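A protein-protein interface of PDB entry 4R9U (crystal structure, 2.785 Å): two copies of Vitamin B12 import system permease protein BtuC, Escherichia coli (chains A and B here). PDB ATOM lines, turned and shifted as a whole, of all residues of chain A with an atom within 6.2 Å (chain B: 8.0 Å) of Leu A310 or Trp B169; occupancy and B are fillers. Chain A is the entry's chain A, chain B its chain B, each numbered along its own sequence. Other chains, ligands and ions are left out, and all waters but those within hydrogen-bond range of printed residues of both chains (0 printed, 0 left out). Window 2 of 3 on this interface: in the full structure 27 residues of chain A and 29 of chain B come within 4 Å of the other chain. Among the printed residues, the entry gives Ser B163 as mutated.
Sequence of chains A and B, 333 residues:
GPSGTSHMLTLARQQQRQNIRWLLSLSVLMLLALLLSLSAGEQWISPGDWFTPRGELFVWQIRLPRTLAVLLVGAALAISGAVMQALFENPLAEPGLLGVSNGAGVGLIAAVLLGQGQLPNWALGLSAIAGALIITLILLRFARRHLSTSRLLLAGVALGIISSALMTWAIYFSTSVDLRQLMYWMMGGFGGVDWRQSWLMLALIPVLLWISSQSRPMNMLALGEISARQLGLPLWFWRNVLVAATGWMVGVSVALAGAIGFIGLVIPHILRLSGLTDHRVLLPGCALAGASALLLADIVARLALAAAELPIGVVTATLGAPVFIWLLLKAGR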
ATOM      1  N   ARG A  66     -30.988 -26.920   0.812  1.00  0.00           N
ATOM      2  CA  ARG A  66     -30.531 -26.185   1.979  1.00  0.00           C
ATOM      3  C   ARG A  66     -29.031 -26.244   2.018  1.00  0.00           C
ATOM      4  O   ARG A  66     -28.398 -25.230   2.251  1.00  0.00           O
ATOM      5  CB  ARG A  66     -31.124 -26.793   3.245  1.00  0.00           C
ATOM      6  CG  ARG A  66     -30.864 -26.067   4.552  1.00  0.00           C
ATOM      7  CD  ARG A  66     -30.754 -27.084   5.668  1.00  0.00           C
ATOM      8  NE  ARG A  66     -30.240 -26.540   6.923  1.00  0.00           N
ATOM      9  CZ  ARG A  66     -30.978 -26.385   8.020  1.00  0.00           C
ATOM     10  NH1 ARG A  66     -32.269 -26.692   8.009  1.00  0.00           N
ATOM     11  NH2 ARG A  66     -30.428 -25.902   9.125  1.00  0.00           N
ATOM     12  N   TYR A 184     -33.671 -15.758  14.528  1.00  0.00           N
ATOM     13  CA  TYR A 184     -33.221 -16.499  13.372  1.00  0.00           C
ATOM     14  C   TYR A 184     -32.795 -15.538  12.261  1.00  0.00           C
ATOM     15  O   TYR A 184     -31.933 -15.875  11.448  1.00  0.00           O
ATOM     16  CB  TYR A 184     -34.286 -17.479  12.892  1.00  0.00           C
ATOM     17  CG  TYR A 184     -34.341 -18.748  13.717  1.00  0.00           C
ATOM     18  CD1 TYR A 184     -33.200 -19.261  14.345  1.00  0.00           C
ATOM     19  CD2 TYR A 184     -35.538 -19.416  13.894  1.00  0.00           C
ATOM     20  CE1 TYR A 184     -33.275 -20.423  15.118  1.00  0.00           C
ATOM     21  CE2 TYR A 184     -35.617 -20.557  14.644  1.00  0.00           C
ATOM     22  CZ  TYR A 184     -34.495 -21.057  15.255  1.00  0.00           C
ATOM     23  OH  TYR A 184     -34.657 -22.199  15.990  1.00  0.00           O
ATOM     24  N   GLY A 188     -28.901 -15.708  11.730  1.00  0.00           N
ATOM     25  CA  GLY A 188     -28.875 -16.508  10.521  1.00  0.00           C
ATOM     26  C   GLY A 188     -29.430 -17.880  10.716  1.00  0.00           C
ATOM     27  O   GLY A 188     -29.424 -18.403  11.826  1.00  0.00           O
ATOM     28  N   GLY A 189     -29.888 -18.484   9.632  1.00  0.00           N
ATOM     29  CA  GLY A 189     -30.449 -19.813   9.720  1.00  0.00           C
ATOM     30  C   GLY A 189     -31.069 -20.186   8.405  1.00  0.00           C
ATOM     31  O   GLY A 189     -31.618 -19.321   7.706  1.00  0.00           O
ATOM     32  N   VAL A 300     -24.479 -28.740  12.215  1.00  0.00           N
ATOM     33  CA  VAL A 300     -24.299 -28.861  13.645  1.00  0.00           C
ATOM     34  C   VAL A 300     -25.286 -27.944  14.306  1.00  0.00           C
ATOM     35  O   VAL A 300     -25.368 -27.878  15.512  1.00  0.00           O
ATOM     36  CB  VAL A 300     -22.822 -28.519  14.064  1.00  0.00           C
ATOM     37  CG1 VAL A 300     -22.574 -28.603  15.550  1.00  0.00           C
ATOM     38  CG2 VAL A 300     -21.844 -29.410  13.326  1.00  0.00           C
ATOM     39  N   ALA A 301     -26.092 -27.252  13.512  1.00  0.00           N
ATOM     40  CA  ALA A 301     -27.039 -26.324  14.107  1.00  0.00           C
ATOM     41  C   ALA A 301     -28.440 -26.817  13.888  1.00  0.00           C
ATOM     42  O   ALA A 301     -29.385 -26.236  14.423  1.00  0.00           O
ATOM     43  CB  ALA A 301     -26.883 -24.954  13.553  1.00  0.00           C
ATOM     44  N   ARG A 302     -28.587 -27.869  13.095  1.00  0.00           N
ATOM     45  CA  ARG A 302     -29.940 -28.328  12.812  1.00  0.00           C
ATOM     46  C   ARG A 302     -30.191 -29.609  13.572  1.00  0.00           C
ATOM     47  O   ARG A 302     -31.318 -29.876  13.967  1.00  0.00           O
ATOM     48  CB  ARG A 302     -30.185 -28.526  11.300  1.00  0.00           C
ATOM     49  CG  ARG A 302     -29.630 -29.790  10.658  1.00  0.00           C
ATOM     50  CD  ARG A 302     -29.857 -29.797   9.147  1.00  0.00           C
ATOM     51  NE  ARG A 302     -29.420 -31.057   8.563  1.00  0.00           N
ATOM     52  CZ  ARG A 302     -28.566 -31.140   7.548  1.00  0.00           C
ATOM     53  NH1 ARG A 302     -28.034 -30.037   7.015  1.00  0.00           N
ATOM     54  NH2 ARG A 302     -28.214 -32.332   7.091  1.00  0.00           N
ATOM     55  N   ALA A 304     -28.397 -30.490  16.451  1.00  0.00           N
ATOM     56  CA  ALA A 304     -27.648 -30.452  17.690  1.00  0.00           C
ATOM     57  C   ALA A 304     -28.590 -30.371  18.864  1.00  0.00           C
ATOM     58  O   ALA A 304     -28.227 -30.677  19.992  1.00  0.00           O
ATOM     59  CB  ALA A 304     -26.712 -29.299  17.705  1.00  0.00           C
ATOM     60  N   LEU A 305     -29.792 -29.900  18.605  1.00  0.00           N
ATOM     61  CA  LEU A 305     -30.746 -29.788  19.679  1.00  0.00           C
ATOM     62  C   LEU A 305     -32.038 -30.433  19.203  1.00  0.00           C
ATOM     63  O   LEU A 305     -32.701 -29.915  18.305  1.00  0.00           O
ATOM     64  CB  LEU A 305     -30.952 -28.321  20.089  1.00  0.00           C
ATOM     65  CG  LEU A 305     -30.705 -28.037  21.576  1.00  0.00           C
ATOM     66  CD1 LEU A 305     -29.273 -28.385  21.944  1.00  0.00           C
ATOM     67  CD2 LEU A 305     -31.061 -26.617  21.979  1.00  0.00           C
ATOM     68  N   ALA A 308     -35.146 -27.845  19.128  1.00  0.00           N
ATOM     69  CA  ALA A 308     -35.343 -26.997  17.956  1.00  0.00           C
ATOM     70  C   ALA A 308     -34.040 -26.792  17.181  1.00  0.00           C
ATOM     71  O   ALA A 308     -33.062 -27.526  17.348  1.00  0.00           O
ATOM     72  CB  ALA A 308     -35.927 -25.655  18.372  1.00  0.00           C
ATOM     73  N   GLU A 309     -34.030 -25.789  16.325  1.00  0.00           N
ATOM     74  CA  GLU A 309     -32.880 -25.548  15.479  1.00  0.00           C
ATOM     75  C   GLU A 309     -32.096 -24.364  15.997  1.00  0.00           C
ATOM     76  O   GLU A 309     -32.669 -23.309  16.220  1.00  0.00           O
ATOM     77  CB  GLU A 309     -33.350 -25.318  14.039  1.00  0.00           C
ATOM     78  CG  GLU A 309     -32.370 -25.836  13.007  1.00  0.00           C
ATOM     79  CD  GLU A 309     -32.964 -25.992  11.603  1.00  0.00           C
ATOM     80  OE1 GLU A 309     -34.149 -26.368  11.458  1.00  0.00           O
ATOM     81  OE2 GLU A 309     -32.222 -25.724  10.633  1.00  0.00           O
ATOM     82  N   LEU A 310     -30.802 -24.535  16.256  1.00  0.00           N
ATOM     83  CA  LEU A 310     -30.008 -23.393  16.717  1.00  0.00           C
ATOM     84  C   LEU A 310     -29.741 -22.439  15.568  1.00  0.00           C
ATOM     85  O   LEU A 310     -29.771 -22.842  14.397  1.00  0.00           O
ATOM     86  CB  LEU A 310     -28.678 -23.841  17.306  1.00  0.00           C
ATOM     87  CG  LEU A 310     -28.641 -24.517  18.668  1.00  0.00           C
ATOM     88  CD1 LEU A 310     -28.781 -26.001  18.473  1.00  0.00           C
ATOM     89  CD2 LEU A 310     -27.363 -24.227  19.422  1.00  0.00           C
ATOM     90  N   PRO A 311     -29.358 -21.202  15.897  1.00  0.00           N
ATOM     91  CA  PRO A 311     -29.028 -20.297  14.799  1.00  0.00           C
ATOM     92  C   PRO A 311     -27.569 -20.337  14.463  1.00  0.00           C
ATOM     93  O   PRO A 311     -26.771 -20.483  15.380  1.00  0.00           O
ATOM     94  CB  PRO A 311     -29.430 -18.937  15.359  1.00  0.00           C
ATOM     95  CG  PRO A 311     -29.400 -19.079  16.838  1.00  0.00           C
ATOM     96  CD  PRO A 311     -29.397 -20.518  17.206  1.00  0.00           C
ATOM     97  N   ILE A 312     -27.207 -20.196  13.202  1.00  0.00           N
ATOM     98  CA  ILE A 312     -25.816 -20.416  12.847  1.00  0.00           C
ATOM     99  C   ILE A 312     -24.871 -19.499  13.614  1.00  0.00           C
ATOM    100  O   ILE A 312     -23.794 -19.944  14.027  1.00  0.00           O
ATOM    101  CB  ILE A 312     -25.588 -20.264  11.387  1.00  0.00           C
ATOM    102  CG1 ILE A 312     -26.749 -20.828  10.626  1.00  0.00           C
ATOM    103  CG2 ILE A 312     -24.384 -21.060  10.977  1.00  0.00           C
ATOM    104  CD1 ILE A 312     -26.427 -20.790   9.216  1.00  0.00           C
ATOM    105  N   VAL A 314     -24.492 -18.937  16.402  1.00  0.00           N
ATOM    106  CA  VAL A 314     -24.062 -19.541  17.642  1.00  0.00           C
ATOM    107  C   VAL A 314     -22.996 -20.537  17.298  1.00  0.00           C
ATOM    108  O   VAL A 314     -21.830 -20.261  17.521  1.00  0.00           O
ATOM    109  CB  VAL A 314     -25.189 -20.241  18.364  1.00  0.00           C
ATOM    110  CG1 VAL A 314     -24.632 -21.062  19.529  1.00  0.00           C
ATOM    111  CG2 VAL A 314     -26.200 -19.231  18.830  1.00  0.00           C
ATOM    112  N   VAL A 315     -23.381 -21.647  16.690  1.00  0.00           N
ATOM    113  CA  VAL A 315     -22.436 -22.714  16.425  1.00  0.00           C
ATOM    114  C   VAL A 315     -21.186 -22.263  15.671  1.00  0.00           C
ATOM    115  O   VAL A 315     -20.072 -22.673  16.016  1.00  0.00           O
ATOM    116  CB  VAL A 315     -23.153 -23.802  15.624  1.00  0.00           C
ATOM    117  CG1 VAL A 315     -23.907 -23.180  14.487  1.00  0.00           C
ATOM    118  CG2 VAL A 315     -22.191 -24.908  15.160  1.00  0.00           C
ATOM    119  N   THR A 318     -19.034 -20.429  18.155  1.00  0.00           N
ATOM    120  CA  THR A 318     -18.825 -21.408  19.213  1.00  0.00           C
ATOM    121  C   THR A 318     -17.701 -22.354  18.860  1.00  0.00           C
ATOM    122  O   THR A 318     -16.904 -22.715  19.715  1.00  0.00           O
ATOM    123  CB  THR A 318     -20.077 -22.238  19.479  1.00  0.00           C
ATOM    124  OG1 THR A 318     -21.102 -21.391  20.019  1.00  0.00           O
ATOM    125  CG2 THR A 318     -19.776 -23.297  20.492  1.00  0.00           C
ATOM    126  N   ILE B 109     -23.201 -13.403  34.515  1.00  0.00           N
ATOM    127  CA  ILE B 109     -24.028 -14.593  34.462  1.00  0.00           C
ATOM    128  C   ILE B 109     -23.489 -15.688  35.380  1.00  0.00           C
ATOM    129  O   ILE B 109     -24.243 -16.322  36.121  1.00  0.00           O
ATOM    130  CB  ILE B 109     -24.094 -15.204  33.086  1.00  0.00           C
ATOM    131  CG1 ILE B 109     -24.610 -14.225  32.053  1.00  0.00           C
ATOM    132  CG2 ILE B 109     -25.055 -16.364  33.135  1.00  0.00           C
ATOM    133  CD1 ILE B 109     -26.076 -13.998  32.183  1.00  0.00           C
ATOM    134  N   LEU B 113     -26.026 -17.622  38.033  1.00  0.00           N
ATOM    135  CA  LEU B 113     -26.115 -19.069  38.061  1.00  0.00           C
ATOM    136  C   LEU B 113     -25.416 -19.692  39.288  1.00  0.00           C
ATOM    137  O   LEU B 113     -26.077 -20.365  40.076  1.00  0.00           O
ATOM    138  CB  LEU B 113     -25.534 -19.637  36.770  1.00  0.00           C
ATOM    139  CG  LEU B 113     -26.289 -19.262  35.488  1.00  0.00           C
ATOM    140  CD1 LEU B 113     -26.024 -20.275  34.375  1.00  0.00           C
ATOM    141  CD2 LEU B 113     -27.786 -19.065  35.723  1.00  0.00           C
ATOM    142  N   ILE B 162     -15.311 -15.550  21.253  1.00  0.00           N
ATOM    143  CA  ILE B 162     -15.460 -16.643  22.232  1.00  0.00           C
ATOM    144  C   ILE B 162     -16.348 -16.256  23.400  1.00  0.00           C
ATOM    145  O   ILE B 162     -17.255 -17.003  23.768  1.00  0.00           O
ATOM    146  CB  ILE B 162     -14.119 -17.042  22.872  1.00  0.00           C
ATOM    147  CG1 ILE B 162     -13.151 -17.660  21.870  1.00  0.00           C
ATOM    148  CG2 ILE B 162     -14.327 -17.973  24.077  1.00  0.00           C
ATOM    149  CD1 ILE B 162     -11.834 -18.031  22.551  1.00  0.00           C
ATOM    150  N   SER B 163     -16.084 -15.105  23.999  1.00  0.00           N
ATOM    151  CA  SER B 163     -16.911 -14.648  25.109  1.00  0.00           C
ATOM    152  C   SER B 163     -18.379 -14.473  24.678  1.00  0.00           C
ATOM    153  O   SER B 163     -19.266 -14.740  25.474  1.00  0.00           O
ATOM    154  CB  SER B 163     -16.358 -13.358  25.712  1.00  0.00           C
ATOM    155  OG  SER B 163     -15.359 -12.832  24.868  1.00  0.00           O
ATOM    156  N   SER B 164     -18.622 -13.976  23.456  1.00  0.00           N
ATOM    157  CA  SER B 164     -19.997 -13.896  22.950  1.00  0.00           C
ATOM    158  C   SER B 164     -20.673 -15.245  22.951  1.00  0.00           C
ATOM    159  O   SER B 164     -21.804 -15.409  23.439  1.00  0.00           O
ATOM    160  CB  SER B 164     -20.032 -13.336  21.535  1.00  0.00           C
ATOM    161  OG  SER B 164     -21.369 -13.050  21.174  1.00  0.00           O
ATOM    162  N   ALA B 165     -19.937 -16.224  22.435  1.00  0.00           N
ATOM    163  CA  ALA B 165     -20.524 -17.539  22.280  1.00  0.00           C
ATOM    164  C   ALA B 165     -20.664 -18.189  23.640  1.00  0.00           C
ATOM    165  O   ALA B 165     -21.494 -19.063  23.819  1.00  0.00           O
ATOM    166  CB  ALA B 165     -19.678 -18.396  21.347  1.00  0.00           C
ATOM    167  N   LEU B 166     -19.915 -17.726  24.630  1.00  0.00           N
ATOM    168  CA  LEU B 166     -20.015 -18.336  25.955  1.00  0.00           C
ATOM    169  C   LEU B 166     -21.165 -17.740  26.726  1.00  0.00           C
ATOM    170  O   LEU B 166     -21.902 -18.428  27.422  1.00  0.00           O
ATOM    171  CB  LEU B 166     -18.735 -18.169  26.754  1.00  0.00           C
ATOM    172  CG  LEU B 166     -17.793 -19.362  26.636  1.00  0.00           C
ATOM    173  CD1 LEU B 166     -16.534 -19.152  27.469  1.00  0.00           C
ATOM    174  CD2 LEU B 166     -18.498 -20.662  27.017  1.00  0.00           C
ATOM    175  N   MET B 167     -21.300 -16.438  26.582  1.00  0.00           N
ATOM    176  CA  MET B 167     -22.311 -15.709  27.301  1.00  0.00           C
ATOM    177  C   MET B 167     -23.668 -16.093  26.750  1.00  0.00           C
ATOM    178  O   MET B 167     -24.659 -16.122  27.472  1.00  0.00           O
ATOM    179  CB  MET B 167     -22.069 -14.209  27.145  1.00  0.00           C
ATOM    180  CG  MET B 167     -22.675 -13.371  28.232  1.00  0.00           C
ATOM    181  SD  MET B 167     -22.908 -11.690  27.643  1.00  0.00           S
ATOM    182  CE  MET B 167     -21.368 -11.419  26.759  1.00  0.00           C
ATOM    183  N   THR B 168     -23.723 -16.450  25.476  1.00  0.00           N
ATOM    184  CA  THR B 168     -25.027 -16.799  24.965  1.00  0.00           C
ATOM    185  C   THR B 168     -25.509 -18.146  25.465  1.00  0.00           C
ATOM    186  O   THR B 168     -26.698 -18.395  25.468  1.00  0.00           O
ATOM    187  CB  THR B 168     -25.065 -16.797  23.459  1.00  0.00           C
ATOM    188  OG1 THR B 168     -26.288 -17.407  23.060  1.00  0.00           O
ATOM    189  CG2 THR B 168     -23.962 -17.628  22.914  1.00  0.00           C
ATOM    190  N   TRP B 169     -24.603 -19.012  25.901  1.00  0.00           N
ATOM    191  CA  TRP B 169     -24.990 -20.354  26.353  1.00  0.00           C
ATOM    192  C   TRP B 169     -25.514 -20.323  27.768  1.00  0.00           C
ATOM    193  O   TRP B 169     -26.459 -21.030  28.132  1.00  0.00           O
ATOM    194  CB  TRP B 169     -23.805 -21.288  26.279  1.00  0.00           C
ATOM    195  CG  TRP B 169     -23.667 -21.885  24.970  1.00  0.00           C
ATOM    196  CD1 TRP B 169     -22.598 -21.782  24.146  1.00  0.00           C
ATOM    197  CD2 TRP B 169     -24.620 -22.706  24.297  1.00  0.00           C
ATOM    198  NE1 TRP B 169     -22.823 -22.472  22.984  1.00  0.00           N
ATOM    199  CE2 TRP B 169     -24.060 -23.054  23.056  1.00  0.00           C
ATOM    200  CE3 TRP B 169     -25.896 -23.182  24.622  1.00  0.00           C
ATOM    201  CZ2 TRP B 169     -24.725 -23.852  22.138  1.00  0.00           C
ATOM    202  CZ3 TRP B 169     -26.555 -23.977  23.707  1.00  0.00           C
ATOM    203  CH2 TRP B 169     -25.969 -24.304  22.483  1.00  0.00           C
ATOM    204  N   ALA B 170     -24.875 -19.495  28.573  1.00  0.00           N
ATOM    205  CA  ALA B 170     -25.257 -19.378  29.960  1.00  0.00           C
ATOM    206  C   ALA B 170     -26.654 -18.780  30.109  1.00  0.00           C
ATOM    207  O   ALA B 170     -27.331 -19.057  31.084  1.00  0.00           O
ATOM    208  CB  ALA B 170     -24.230 -18.541  30.746  1.00  0.00           C
ATOM    209  N   ILE B 171     -27.052 -17.927  29.163  1.00  0.00           N
ATOM    210  CA  ILE B 171     -28.367 -17.304  29.191  1.00  0.00           C
ATOM    211  C   ILE B 171     -29.427 -18.351  28.843  1.00  0.00           C
ATOM    212  O   ILE B 171     -30.605 -18.204  29.156  1.00  0.00           O
ATOM    213  CB  ILE B 171     -28.426 -16.108  28.197  1.00  0.00           C
ATOM    214  CG1 ILE B 171     -27.423 -15.016  28.562  1.00  0.00           C
ATOM    215  CG2 ILE B 171     -29.763 -15.455  28.193  1.00  0.00           C
ATOM    216  CD1 ILE B 171     -27.464 -13.824  27.618  1.00  0.00           C
ATOM    217  N   TYR B 172     -28.978 -19.457  28.275  1.00  0.00           N
ATOM    218  CA  TYR B 172     -29.893 -20.515  27.871  1.00  0.00           C
ATOM    219  C   TYR B 172     -30.306 -21.406  29.067  1.00  0.00           C
ATOM    220  O   TYR B 172     -31.389 -21.984  29.070  1.00  0.00           O
ATOM    221  CB  TYR B 172     -29.226 -21.340  26.768  1.00  0.00           C
ATOM    222  CG  TYR B 172     -29.974 -22.564  26.322  1.00  0.00           C
ATOM    223  CD1 TYR B 172     -29.442 -23.833  26.547  1.00  0.00           C
ATOM    224  CD2 TYR B 172     -31.235 -22.455  25.692  1.00  0.00           C
ATOM    225  CE1 TYR B 172     -30.098 -24.956  26.159  1.00  0.00           C
ATOM    226  CE2 TYR B 172     -31.915 -23.577  25.292  1.00  0.00           C
ATOM    227  CZ  TYR B 172     -31.334 -24.830  25.531  1.00  0.00           C
ATOM    228  OH  TYR B 172     -31.956 -26.000  25.158  1.00  0.00           O
ATOM    229  N   PHE B 173     -29.476 -21.470  30.104  1.00  0.00           N
ATOM    230  CA  PHE B 173     -29.790 -22.291  31.274  1.00  0.00           C
ATOM    231  C   PHE B 173     -30.173 -21.481  32.498  1.00  0.00           C
ATOM    232  O   PHE B 173     -29.839 -21.856  33.616  1.00  0.00           O
ATOM    233  CB  PHE B 173     -28.603 -23.170  31.658  1.00  0.00           C
ATOM    234  CG  PHE B 173     -28.030 -23.967  30.523  1.00  0.00           C
ATOM    235  CD1 PHE B 173     -26.767 -23.655  30.028  1.00  0.00           C
ATOM    236  CD2 PHE B 173     -28.731 -25.044  29.976  1.00  0.00           C
ATOM    237  CE1 PHE B 173     -26.218 -24.399  28.991  1.00  0.00           C
ATOM    238  CE2 PHE B 173     -28.197 -25.799  28.933  1.00  0.00           C
ATOM    239  CZ  PHE B 173     -26.937 -25.478  28.440  1.00  0.00           C
ATOM    240  N   SER B 174     -30.865 -20.377  32.322  1.00  0.00           N
ATOM    241  CA  SER B 174     -31.108 -19.523  33.464  1.00  0.00           C
ATOM    242  C   SER B 174     -32.571 -19.211  33.600  1.00  0.00           C
ATOM    243  O   SER B 174     -33.239 -18.936  32.608  1.00  0.00           O
ATOM    244  CB  SER B 174     -30.275 -18.256  33.339  1.00  0.00           C
ATOM    245  OG  SER B 174     -29.833 -18.122  32.000  1.00  0.00           O
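No position is printed for both chains. Of the 5 pairs that touch across the chains among the printed residues, none has its exchanged pair printed and touching as well.
Trp B169 touches just these residues of chain A: Leu A310, Val A314 and Thr A318. No residue of chain B comes within 4 Å of Pro A311. Printed residues of chain B within 4 Å of Leu A305: Tyr B172. Of the printed residues of chain B, Val A314 touches Trp B169 (3.8 Å). The nearest residue of chain B that does not touch Leu A310 is Tyr B172 (7.3 Å). The nearest residue of chain A that does not touch Trp B169 is Leu A305 (5.3 Å).
Hydrophobic or aromatic side chains of chain A within 4 Å of the printed part of chain B: Leu A305, Leu A310 and Val A314. Hydrophobic or aromatic side chains of chain B within 4 Å of the printed part of chain A: Ala B165, Trp B169 and Tyr B172. Among the printed residues, 5 pairs touch across the chains.
O of Ala A301 lies within hydrogen-bond range of N of Leu A310 (2.9 Å). The side-chain hydroxyl (OG1) of Thr A318 sits at hydrogen-bond distance from the backbone carbonyl oxygen (O) of Val A314 (2.8 Å).
Among the printed residues, merely in contact across the chains: Leu A305 with Tyr B172, Leu A310 with Trp B169, Val A314 with Trp B169, Thr A318 with Ala B165 and Thr A318 with Trp B169.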
